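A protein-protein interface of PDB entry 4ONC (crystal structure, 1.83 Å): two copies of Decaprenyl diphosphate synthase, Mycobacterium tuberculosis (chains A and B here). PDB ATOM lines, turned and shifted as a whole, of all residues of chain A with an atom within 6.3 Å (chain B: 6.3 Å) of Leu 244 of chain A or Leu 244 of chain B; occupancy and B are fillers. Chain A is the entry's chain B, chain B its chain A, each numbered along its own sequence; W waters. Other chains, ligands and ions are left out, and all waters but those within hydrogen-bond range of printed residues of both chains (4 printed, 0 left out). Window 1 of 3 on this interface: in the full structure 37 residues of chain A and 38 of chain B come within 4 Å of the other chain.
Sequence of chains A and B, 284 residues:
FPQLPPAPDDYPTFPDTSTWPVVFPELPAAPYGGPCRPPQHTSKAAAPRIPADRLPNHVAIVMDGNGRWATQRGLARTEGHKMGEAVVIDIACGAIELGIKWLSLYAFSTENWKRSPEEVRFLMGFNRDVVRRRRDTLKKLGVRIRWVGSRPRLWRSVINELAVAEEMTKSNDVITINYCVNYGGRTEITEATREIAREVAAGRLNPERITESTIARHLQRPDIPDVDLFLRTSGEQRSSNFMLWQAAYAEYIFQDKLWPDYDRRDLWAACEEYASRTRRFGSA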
ATOM      1  N   TYR A 183     -34.213  -2.026  12.879  1.00  0.00           N
ATOM      2  CA  TYR A 183     -33.389  -1.727  11.701  1.00  0.00           C
ATOM      3  C   TYR A 183     -33.163  -0.235  11.625  1.00  0.00           C
ATOM      4  O   TYR A 183     -34.082   0.601  11.891  1.00  0.00           O
ATOM      5  CB  TYR A 183     -34.152  -2.233  10.466  1.00  0.00           C
ATOM      6  CG  TYR A 183     -33.342  -1.823   9.207  1.00  0.00           C
ATOM      7  CD1 TYR A 183     -33.379  -0.479   8.780  1.00  0.00           C
ATOM      8  CD2 TYR A 183     -32.431  -2.727   8.617  1.00  0.00           C
ATOM      9  CE1 TYR A 183     -32.539  -0.041   7.715  1.00  0.00           C
ATOM     10  CE2 TYR A 183     -31.644  -2.309   7.514  1.00  0.00           C
ATOM     11  CZ  TYR A 183     -31.697  -0.978   7.111  1.00  0.00           C
ATOM     12  OH  TYR A 183     -30.897  -0.530   6.052  1.00  0.00           O
ATOM     13  N   GLY A 184     -31.895   0.153  11.337  1.00  0.00           N
ATOM     14  CA  GLY A 184     -31.613   1.613  11.096  1.00  0.00           C
ATOM     15  C   GLY A 184     -30.483   1.603  10.030  1.00  0.00           C
ATOM     16  O   GLY A 184     -29.491   0.796  10.163  1.00  0.00           O
ATOM     17  N   GLY A 185     -30.622   2.415   8.949  1.00  0.00           N
ATOM     18  CA  GLY A 185     -29.666   2.258   7.830  1.00  0.00           C
ATOM     19  C   GLY A 185     -28.253   2.678   8.272  1.00  0.00           C
ATOM     20  O   GLY A 185     -27.243   2.005   7.931  1.00  0.00           O
ATOM     21  N   ARG A 186     -28.162   3.820   8.954  1.00  0.00           N
ATOM     22  CA  ARG A 186     -26.810   4.238   9.490  1.00  0.00           C
ATOM     23  C   ARG A 186     -26.218   3.227  10.412  1.00  0.00           C
ATOM     24  O   ARG A 186     -25.016   2.955  10.307  1.00  0.00           O
ATOM     25  CB  ARG A 186     -26.899   5.520  10.285  1.00  0.00           C
ATOM     26  CG  ARG A 186     -27.239   6.741   9.419  1.00  0.00           C
ATOM     27  CD  ARG A 186     -27.184   7.984  10.295  1.00  0.00           C
ATOM     28  NE  ARG A 186     -27.381   9.249   9.540  1.00  0.00           N
ATOM     29  CZ  ARG A 186     -27.558  10.429  10.146  1.00  0.00           C
ATOM     30  NH1 ARG A 186     -27.636  10.485  11.492  1.00  0.00           N
ATOM     31  NH2 ARG A 186     -27.730  11.556   9.460  1.00  0.00           N
ATOM     32  N   GLU A 188     -26.711  -0.147  10.371  1.00  0.00           N
ATOM     33  CA  GLU A 188     -26.351  -1.315   9.588  1.00  0.00           C
ATOM     34  C   GLU A 188     -24.977  -0.987   8.867  1.00  0.00           C
ATOM     35  O   GLU A 188     -24.065  -1.840   8.813  1.00  0.00           O
ATOM     36  CB  GLU A 188     -27.486  -1.528   8.558  1.00  0.00           C
ATOM     37  CG  GLU A 188     -27.102  -2.453   7.443  1.00  0.00           C
ATOM     38  CD  GLU A 188     -28.259  -2.783   6.591  1.00  0.00           C
ATOM     39  OE1 GLU A 188     -28.773  -1.939   5.787  1.00  0.00           O
ATOM     40  OE2 GLU A 188     -28.668  -3.877   6.781  1.00  0.00           O
ATOM     41  N   ILE A 189     -24.861   0.221   8.343  1.00  0.00           N
ATOM     42  CA  ILE A 189     -23.546   0.640   7.744  1.00  0.00           C
ATOM     43  C   ILE A 189     -22.411   0.674   8.809  1.00  0.00           C
ATOM     44  O   ILE A 189     -21.264   0.186   8.562  1.00  0.00           O
ATOM     45  CB  ILE A 189     -23.717   2.021   7.056  1.00  0.00           C
ATOM     46  CG1 ILE A 189     -24.599   1.882   5.749  1.00  0.00           C
ATOM     47  CG2 ILE A 189     -22.313   2.606   6.693  1.00  0.00           C
ATOM     48  CD1 ILE A 189     -25.240   3.258   5.295  1.00  0.00           C
ATOM     49  N   SER A 239     -37.433   8.951   3.853  1.00  0.00           N
ATOM     50  CA  SER A 239     -36.999   7.546   3.746  1.00  0.00           C
ATOM     51  C   SER A 239     -36.782   6.975   5.212  1.00  0.00           C
ATOM     52  O   SER A 239     -36.712   5.775   5.355  1.00  0.00           O
ATOM     53  CB  SER A 239     -35.676   7.375   2.975  1.00  0.00           C
ATOM     54  OG  SER A 239     -34.657   7.922   3.776  1.00  0.00           O
ATOM     55  N   ASN A 241     -34.384   6.569   7.139  1.00  0.00           N
ATOM     56  CA  ASN A 241     -33.209   5.709   7.494  1.00  0.00           C
ATOM     57  C   ASN A 241     -33.462   4.267   7.134  1.00  0.00           C
ATOM     58  O   ASN A 241     -32.756   3.353   7.609  1.00  0.00           O
ATOM     59  CB  ASN A 241     -32.840   5.919   8.997  1.00  0.00           C
ATOM     60  CG  ASN A 241     -31.453   5.428   9.369  1.00  0.00           C
ATOM     61  OD1 ASN A 241     -30.512   5.447   8.545  1.00  0.00           O
ATOM     62  ND2 ASN A 241     -31.303   4.965  10.636  1.00  0.00           N
ATOM     63  N   PHE A 242     -34.437   4.014   6.227  1.00  0.00           N
ATOM     64  CA  PHE A 242     -34.703   2.624   5.888  1.00  0.00           C
ATOM     65  C   PHE A 242     -33.923   2.146   4.629  1.00  0.00           C
ATOM     66  O   PHE A 242     -33.960   2.858   3.592  1.00  0.00           O
ATOM     67  CB  PHE A 242     -36.219   2.473   5.633  1.00  0.00           C
ATOM     68  CG  PHE A 242     -36.674   1.061   5.464  1.00  0.00           C
ATOM     69  CD1 PHE A 242     -36.170   0.075   6.268  1.00  0.00           C
ATOM     70  CD2 PHE A 242     -37.602   0.703   4.471  1.00  0.00           C
ATOM     71  CE1 PHE A 242     -36.576  -1.263   6.109  1.00  0.00           C
ATOM     72  CE2 PHE A 242     -38.043  -0.611   4.340  1.00  0.00           C
ATOM     73  CZ  PHE A 242     -37.503  -1.613   5.102  1.00  0.00           C
ATOM     74  N   MET A 243     -33.240   1.007   4.702  1.00  0.00           N
ATOM     75  CA  MET A 243     -32.483   0.504   3.561  1.00  0.00           C
ATOM     76  C   MET A 243     -31.546   1.585   3.023  1.00  0.00           C
ATOM     77  O   MET A 243     -31.497   1.847   1.860  1.00  0.00           O
ATOM     78  CB  MET A 243     -33.409   0.040   2.447  1.00  0.00           C
ATOM     79  CG  MET A 243     -34.055  -1.294   2.647  1.00  0.00           C
ATOM     80  SD  MET A 243     -32.965  -2.707   2.839  1.00  0.00           S
ATOM     81  CE  MET A 243     -33.740  -3.268   4.299  1.00  0.00           C
ATOM     82  N   LEU A 244     -30.813   2.209   3.897  1.00  0.00           N
ATOM     83  CA  LEU A 244     -30.154   3.440   3.509  1.00  0.00           C
ATOM     84  C   LEU A 244     -29.097   3.175   2.414  1.00  0.00           C
ATOM     85  O   LEU A 244     -29.121   3.857   1.385  1.00  0.00           O
ATOM     86  CB  LEU A 244     -29.532   4.126   4.751  1.00  0.00           C
ATOM     87  CG  LEU A 244     -28.740   5.416   4.459  1.00  0.00           C
ATOM     88  CD1 LEU A 244     -29.758   6.508   4.094  1.00  0.00           C
ATOM     89  CD2 LEU A 244     -28.128   5.815   5.813  1.00  0.00           C
ATOM     90  N   TRP A 245     -28.217   2.202   2.609  1.00  0.00           N
ATOM     91  CA  TRP A 245     -27.229   1.878   1.554  1.00  0.00           C
ATOM     92  C   TRP A 245     -27.915   1.346   0.306  1.00  0.00           C
ATOM     93  O   TRP A 245     -27.631   1.783  -0.826  1.00  0.00           O
ATOM     94  CB  TRP A 245     -26.301   0.782   2.121  1.00  0.00           C
ATOM     95  CG  TRP A 245     -25.227   0.420   1.132  1.00  0.00           C
ATOM     96  CD1 TRP A 245     -25.264  -0.572   0.149  1.00  0.00           C
ATOM     97  CD2 TRP A 245     -23.907   1.030   1.037  1.00  0.00           C
ATOM     98  NE1 TRP A 245     -24.059  -0.591  -0.567  1.00  0.00           N
ATOM     99  CE2 TRP A 245     -23.220   0.338  -0.080  1.00  0.00           C
ATOM    100  CE3 TRP A 245     -23.267   2.108   1.692  1.00  0.00           C
ATOM    101  CZ2 TRP A 245     -21.896   0.640  -0.461  1.00  0.00           C
ATOM    102  CZ3 TRP A 245     -21.899   2.408   1.276  1.00  0.00           C
ATOM    103  CH2 TRP A 245     -21.291   1.693   0.172  1.00  0.00           C
ATOM    104  N   GLN A 246     -28.930   0.452   0.473  1.00  0.00           N
ATOM    105  CA  GLN A 246     -29.507  -0.283  -0.642  1.00  0.00           C
ATOM    106  C   GLN A 246     -30.424   0.576  -1.493  1.00  0.00           C
ATOM    107  O   GLN A 246     -30.592   0.228  -2.681  1.00  0.00           O
ATOM    108  CB  GLN A 246     -30.316  -1.552  -0.182  1.00  0.00           C
ATOM    109  CG  GLN A 246     -29.462  -2.512   0.725  1.00  0.00           C
ATOM    110  CD  GLN A 246     -29.480  -2.101   2.247  1.00  0.00           C
ATOM    111  OE1 GLN A 246     -29.742  -1.007   2.614  1.00  0.00           O
ATOM    112  NE2 GLN A 246     -29.111  -3.033   3.096  1.00  0.00           N
ATOM    113  N   ALA A 247     -30.984   1.670  -0.928  1.00  0.00           N
ATOM    114  CA  ALA A 247     -32.005   2.478  -1.617  1.00  0.00           C
ATOM    115  C   ALA A 247     -31.372   3.741  -2.201  1.00  0.00           C
ATOM    116  O   ALA A 247     -32.059   4.710  -2.559  1.00  0.00           O
ATOM    117  CB  ALA A 247     -33.199   2.871  -0.666  1.00  0.00           C
ATOM    118  N   ALA A 248     -30.017   3.789  -2.257  1.00  0.00           N
ATOM    119  CA  ALA A 248     -29.379   5.058  -2.630  1.00  0.00           C
ATOM    120  C   ALA A 248     -29.866   5.544  -4.017  1.00  0.00           C
ATOM    121  O   ALA A 248     -30.001   6.752  -4.231  1.00  0.00           O
ATOM    122  CB  ALA A 248     -27.843   4.809  -2.694  1.00  0.00           C
ATOM    123  N   TYR B 183     -19.319  13.982  -6.270  1.00  0.00           N
ATOM    124  CA  TYR B 183     -19.817  13.543  -4.982  1.00  0.00           C
ATOM    125  C   TYR B 183     -20.683  12.266  -5.193  1.00  0.00           C
ATOM    126  O   TYR B 183     -21.476  12.209  -6.162  1.00  0.00           O
ATOM    127  CB  TYR B 183     -20.631  14.675  -4.365  1.00  0.00           C
ATOM    128  CG  TYR B 183     -21.319  14.201  -3.099  1.00  0.00           C
ATOM    129  CD1 TYR B 183     -22.518  13.429  -3.159  1.00  0.00           C
ATOM    130  CD2 TYR B 183     -20.728  14.439  -1.802  1.00  0.00           C
ATOM    131  CE1 TYR B 183     -23.076  12.861  -2.016  1.00  0.00           C
ATOM    132  CE2 TYR B 183     -21.318  13.892  -0.650  1.00  0.00           C
ATOM    133  CZ  TYR B 183     -22.463  13.078  -0.763  1.00  0.00           C
ATOM    134  OH  TYR B 183     -23.077  12.490   0.345  1.00  0.00           O
ATOM    135  N   GLY B 184     -20.563  11.284  -4.279  1.00  0.00           N
ATOM    136  CA  GLY B 184     -21.509  10.121  -4.303  1.00  0.00           C
ATOM    137  C   GLY B 184     -21.612   9.712  -2.869  1.00  0.00           C
ATOM    138  O   GLY B 184     -20.618   9.613  -2.168  1.00  0.00           O
ATOM    139  N   GLY B 185     -22.818   9.442  -2.423  1.00  0.00           N
ATOM    140  CA  GLY B 185     -23.056   9.248  -0.989  1.00  0.00           C
ATOM    141  C   GLY B 185     -22.426   7.917  -0.510  1.00  0.00           C
ATOM    142  O   GLY B 185     -21.756   7.895   0.532  1.00  0.00           O
ATOM    143  N   ARG B 186     -22.616   6.823  -1.238  1.00  0.00           N
ATOM    144  CA  ARG B 186     -21.953   5.607  -0.860  1.00  0.00           C
ATOM    145  C   ARG B 186     -20.448   5.809  -0.883  1.00  0.00           C
ATOM    146  O   ARG B 186     -19.711   5.226  -0.064  1.00  0.00           O
ATOM    147  CB  ARG B 186     -22.318   4.529  -1.875  1.00  0.00           C
ATOM    148  CG  ARG B 186     -23.780   3.992  -1.702  1.00  0.00           C
ATOM    149  CD  ARG B 186     -23.918   2.861  -2.737  1.00  0.00           C
ATOM    150  NE  ARG B 186     -25.235   2.201  -2.564  1.00  0.00           N
ATOM    151  CZ  ARG B 186     -25.616   1.253  -3.382  1.00  0.00           C
ATOM    152  NH1 ARG B 186     -24.821   0.902  -4.416  1.00  0.00           N
ATOM    153  NH2 ARG B 186     -26.830   0.721  -3.285  1.00  0.00           N
ATOM    154  N   GLU B 188     -18.668   8.478  -0.376  1.00  0.00           N
ATOM    155  CA  GLU B 188     -18.234   9.271   0.764  1.00  0.00           C
ATOM    156  C   GLU B 188     -18.215   8.413   2.092  1.00  0.00           C
ATOM    157  O   GLU B 188     -17.302   8.540   2.916  1.00  0.00           O
ATOM    158  CB  GLU B 188     -19.271  10.434   0.862  1.00  0.00           C
ATOM    159  CG  GLU B 188     -19.213  11.144   2.127  1.00  0.00           C
ATOM    160  CD  GLU B 188     -20.104  12.320   2.188  1.00  0.00           C
ATOM    161  OE1 GLU B 188     -21.350  12.152   2.311  1.00  0.00           O
ATOM    162  OE2 GLU B 188     -19.559  13.438   2.165  1.00  0.00           O
ATOM    163  N   ILE B 189     -19.180   7.501   2.244  1.00  0.00           N
ATOM    164  CA  ILE B 189     -19.237   6.643   3.410  1.00  0.00           C
ATOM    165  C   ILE B 189     -18.108   5.644   3.276  1.00  0.00           C
ATOM    166  O   ILE B 189     -17.419   5.296   4.278  1.00  0.00           O
ATOM    167  CB  ILE B 189     -20.626   5.926   3.457  1.00  0.00           C
ATOM    168  CG1 ILE B 189     -21.709   6.950   3.905  1.00  0.00           C
ATOM    169  CG2 ILE B 189     -20.544   4.660   4.320  1.00  0.00           C
ATOM    170  CD1 ILE B 189     -23.183   6.642   3.511  1.00  0.00           C
ATOM    171  N   SER B 239     -33.282  10.152  -4.663  1.00  0.00           N
ATOM    172  CA  SER B 239     -32.292  11.004  -3.985  1.00  0.00           C
ATOM    173  C   SER B 239     -30.962  10.880  -4.770  1.00  0.00           C
ATOM    174  O   SER B 239     -30.096  11.719  -4.581  1.00  0.00           O
ATOM    175  CB  SER B 239     -32.022  10.518  -2.532  1.00  0.00           C
ATOM    176  OG  SER B 239     -31.371   9.247  -2.542  1.00  0.00           O
ATOM    177  N   ASN B 241     -28.367   9.110  -4.424  1.00  0.00           N
ATOM    178  CA  ASN B 241     -27.096   8.913  -3.698  1.00  0.00           C
ATOM    179  C   ASN B 241     -26.556  10.283  -3.239  1.00  0.00           C
ATOM    180  O   ASN B 241     -25.371  10.347  -2.918  1.00  0.00           O
ATOM    181  CB  ASN B 241     -26.030   8.284  -4.666  1.00  0.00           C
ATOM    182  CG  ASN B 241     -24.838   7.624  -3.971  1.00  0.00           C
ATOM    183  OD1 ASN B 241     -24.940   7.131  -2.845  1.00  0.00           O
ATOM    184  ND2 ASN B 241     -23.733   7.490  -4.707  1.00  0.00           N
ATOM    185  N   PHE B 242     -27.391  11.337  -3.177  1.00  0.00           N
ATOM    186  CA  PHE B 242     -26.915  12.626  -2.725  1.00  0.00           C
ATOM    187  C   PHE B 242     -27.098  12.805  -1.192  1.00  0.00           C
ATOM    188  O   PHE B 242     -28.212  12.482  -0.637  1.00  0.00           O
ATOM    189  CB  PHE B 242     -27.721  13.747  -3.431  1.00  0.00           C
ATOM    190  CG  PHE B 242     -27.205  15.170  -3.120  1.00  0.00           C
ATOM    191  CD1 PHE B 242     -25.811  15.394  -3.136  1.00  0.00           C
ATOM    192  CD2 PHE B 242     -28.074  16.230  -2.851  1.00  0.00           C
ATOM    193  CE1 PHE B 242     -25.306  16.649  -2.922  1.00  0.00           C
ATOM    194  CE2 PHE B 242     -27.590  17.523  -2.629  1.00  0.00           C
ATOM    195  CZ  PHE B 242     -26.215  17.730  -2.618  1.00  0.00           C
ATOM    196  N   MET B 243     -26.042  13.221  -0.504  1.00  0.00           N
ATOM    197  CA  MET B 243     -26.057  13.436   0.940  1.00  0.00           C
ATOM    198  C   MET B 243     -26.615  12.174   1.639  1.00  0.00           C
ATOM    199  O   MET B 243     -27.437  12.251   2.492  1.00  0.00           O
ATOM    200  CB  MET B 243     -26.937  14.617   1.299  1.00  0.00           C
ATOM    201  CG  MET B 243     -26.372  15.978   1.166  1.00  0.00           C
ATOM    202  SD  MET B 243     -24.817  16.388   1.948  1.00  0.00           S
ATOM    203  CE  MET B 243     -24.203  16.177   0.361  1.00  0.00           C
ATOM    204  N   LEU B 244     -26.139  11.037   1.218  1.00  0.00           N
ATOM    205  CA  LEU B 244     -26.733   9.773   1.619  1.00  0.00           C
ATOM    206  C   LEU B 244     -26.781   9.646   3.184  1.00  0.00           C
ATOM    207  O   LEU B 244     -27.853   9.382   3.771  1.00  0.00           O
ATOM    208  CB  LEU B 244     -25.976   8.576   0.991  1.00  0.00           C
ATOM    209  CG  LEU B 244     -26.644   7.220   1.255  1.00  0.00           C
ATOM    210  CD1 LEU B 244     -28.131   7.193   0.743  1.00  0.00           C
ATOM    211  CD2 LEU B 244     -25.878   6.007   0.610  1.00  0.00           C
ATOM    212  N   TRP B 245     -25.618   9.727   3.805  1.00  0.00           N
ATOM    213  CA  TRP B 245     -25.634   9.663   5.282  1.00  0.00           C
ATOM    214  C   TRP B 245     -26.476  10.781   5.919  1.00  0.00           C
ATOM    215  O   TRP B 245     -27.246  10.560   6.881  1.00  0.00           O
ATOM    216  CB  TRP B 245     -24.160   9.744   5.722  1.00  0.00           C
ATOM    217  CG  TRP B 245     -24.027   9.642   7.203  1.00  0.00           C
ATOM    218  CD1 TRP B 245     -23.970  10.668   8.121  1.00  0.00           C
ATOM    219  CD2 TRP B 245     -23.846   8.401   7.944  1.00  0.00           C
ATOM    220  NE1 TRP B 245     -23.835  10.161   9.422  1.00  0.00           N
ATOM    221  CE2 TRP B 245     -23.755   8.790   9.372  1.00  0.00           C
ATOM    222  CE3 TRP B 245     -23.775   7.073   7.584  1.00  0.00           C
ATOM    223  CZ2 TRP B 245     -23.503   7.843  10.368  1.00  0.00           C
ATOM    224  CZ3 TRP B 245     -23.602   6.087   8.628  1.00  0.00           C
ATOM    225  CH2 TRP B 245     -23.411   6.507   9.958  1.00  0.00           C
ATOM    226  N   GLN B 246     -26.247  12.009   5.452  1.00  0.00           N
ATOM    227  CA  GLN B 246     -26.748  13.192   6.106  1.00  0.00           C
ATOM    228  C   GLN B 246     -28.266  13.345   5.917  1.00  0.00           C
ATOM    229  O   GLN B 246     -28.917  13.995   6.737  1.00  0.00           O
ATOM    230  CB  GLN B 246     -26.066  14.439   5.503  1.00  0.00           C
ATOM    231  CG  GLN B 246     -24.542  14.389   5.659  1.00  0.00           C
ATOM    232  CD  GLN B 246     -23.839  13.763   4.467  1.00  0.00           C
ATOM    233  OE1 GLN B 246     -24.432  12.993   3.695  1.00  0.00           O
ATOM    234  NE2 GLN B 246     -22.516  14.011   4.335  1.00  0.00           N
ATOM    235  N   ALA B 247     -28.841  12.757   4.854  1.00  0.00           N
ATOM    236  CA  ALA B 247     -30.281  12.985   4.592  1.00  0.00           C
ATOM    237  C   ALA B 247     -31.157  11.776   5.030  1.00  0.00           C
ATOM    238  O   ALA B 247     -32.342  11.652   4.662  1.00  0.00           O
ATOM    239  CB  ALA B 247     -30.447  13.287   3.051  1.00  0.00           C
ATOM    240  N   ALA B 248     -30.565  10.848   5.828  1.00  0.00           N
ATOM    241  CA  ALA B 248     -31.287   9.639   6.273  1.00  0.00           C
ATOM    242  C   ALA B 248     -32.635  10.001   6.902  1.00  0.00           C
ATOM    243  O   ALA B 248     -33.577   9.259   6.698  1.00  0.00           O
ATOM    244  CB  ALA B 248     -30.422   8.894   7.333  1.00  0.00           C
HETATM  245  O   HOH W   1     -35.735  10.469   5.247  1.00  0.00           O
HETATM  246  O   HOH W   2     -33.120   9.525   2.737  1.00  0.00           O
HETATM  247  O   HOH W   3     -32.690   7.471  -4.944  1.00  0.00           O
HETATM  248  O   HOH W   4     -32.200   7.235  -1.262  1.00  0.00           O
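Of the 15 printed residues of chain A, 8 touch a printed residue of chain B.
Printed residues of chain A that touch a printed residue of chain B: Arg 186, Ile 189, Ser 239, Asn 241, Leu 244, Trp 245, Gln 246 and Ala 248.
Of the 15 printed residues of chain B, 8 touch a printed residue of chain A.
Hydrophobic or aromatic side chains of chain B that line the printed part of chain A: Ile 189, Leu 244, Trp 245 and Ala 248.
Along chain B the printed residues that touch a printed residue of chain A span positions 186 to 248.
Among the printed residues, 12 pairs touch across the chains.
Among the printed residues, no Asp or Glu carboxylate lies within 4 Å of a Lys or Arg side-chain nitrogen of the other chain.
Water W2 lies within hydrogen-bond range of the side-chain hydroxyl of Ser 239 of chain A (2.5 Å) and the backbone carbonyl oxygen of Ala 247 of chain B (3.0 Å).
Water W4 bridges the side-chain hydroxyl (OG) of Ser 239 of chain B (2.5 Å) and the backbone carbonyl oxygen (O) of Ala 247 of chain A (2.8 Å).
Water W1 lies within hydrogen-bond range of N of Ser 239 of chain A and O of Ala 248 of chain B.
Water W3 lies within hydrogen-bond range of N of Ser 239 of chain B (2.8 Å) and O of Ala 248 of chain A (2.9 Å).
The backbone carbonyl oxygen of Ala 248 of chain B lies within hydrogen-bond range of the side-chain hydroxyl of Ser 239 of chain A, 3.4 Å away.
The backbone NH (N) of Asn 241 of chain B is in hydrogen-bond range of the backbone carbonyl oxygen (O) of Ala 248 of chain A (2.9 Å).
The side-chain hydroxyl (OG) of Ser 239 of chain B sits at hydrogen-bond distance from the backbone carbonyl oxygen (O) of Ala 248 of chain A, 3.3 Å away.
The backbone carbonyl oxygen of Ala 248 of chain B is in hydrogen-bond range of the backbone NH of Asn 241 of chain A, 2.8 Å away.
The backbone carbonyl oxygen (O) of Trp 245 of chain B is in hydrogen-bond range of the guanidinium group (NH2) of Arg 186 of chain A.
The guanidinium group (NH2) of Arg 186 of chain B is in hydrogen-bond range of the backbone carbonyl oxygen (O) of Trp 245 of chain A (2.8 Å).
NH2 of Arg 186 of chain A touches O of Gln 246 of chain B, 3.8 Å away.
Arg 186 of chain A touches Ala 248 of chain B (NE to CB, 3.8 Å).
Ile 189 of chain B touches Ile 189 of chain A (CG2 to CG2, 3.6 Å).
Leu 244 of chain A touches Leu 244 of chain B (CD1 to O, 3.5 Å).
Arg 186 of chain B touches Gln 246 of chain A.
Ala 248 of chain A touches Arg 186 of chain B (CB to NE, 3.7 Å).
Arg 186 of chain A touches Trp 245 of chain B, and with the chains exchanged Trp 245 of chain A touches Arg 186 of chain B.
Arg 186 of chain A touches Gln 246 of chain B, and with the chains exchanged Gln 246 of chain A touches Arg 186 of chain B.
Arg 186 of chain A touches Ala 248 of chain B, and with the chains exchanged Ala 248 of chain A touches Arg 186 of chain B.
Ser 239 of chain A touches Ala 248 of chain B, and with the chains exchanged Ala 248 of chain A touches Ser 239 of chain B.
Of the printed residues of chain B, Ser 239 of chain A touches Ala 248.
Phe 242 of chain A touches none of the printed residues of chain B.
Leu 244 of chain A touches just one residue of chain B: Leu 244.
Of the printed residues of chain B, Trp 245 of chain A touches Arg 186.
Printed residues of chain B within 4 Å of Ala 248 of chain A: Arg 186 (3.7 Å), Ser 239 (3.3 Å) and Asn 241 (2.9 Å).
Of chain A, only Leu 244 (3.5 Å) comes within 4 Å of Leu 244 of chain B.
The nearest residue of chain B that does not touch Leu 244 of chain A is Ala 248 of chain B (4.1 Å).
N of Gly 185 of chain A lies within hydrogen-bond range of O of Asn 241 of chain A, at 2.7 Å.
The side-chain carboxylate of Glu 188 of chain B is in hydrogen-bond range of the side-chain amide nitrogen of Gln 246 of chain B (3.0 Å).
The backbone carbonyl oxygen (O) of Met 243 of chain B sits close to the side-chain amide oxygen (OE1) of Gln 246 of chain B, 3.3 Å away.
The backbone carbonyl oxygen (O) of Met 243 of chain A lies close to the side-chain amide oxygen (OE1) of Gln 246 of chain A (3.4 Å).
The side-chain amide oxygen (OD1) of Asn 241 of chain A sits at hydrogen-bond distance from the backbone NH (N) of Arg 186 of chain A, at 2.9 Å.
The side-chain carboxylate (OE1) of Glu 188 of chain A lies within hydrogen-bond range of the side-chain amide nitrogen (NE2) of Gln 246 of chain A, 2.9 Å away.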
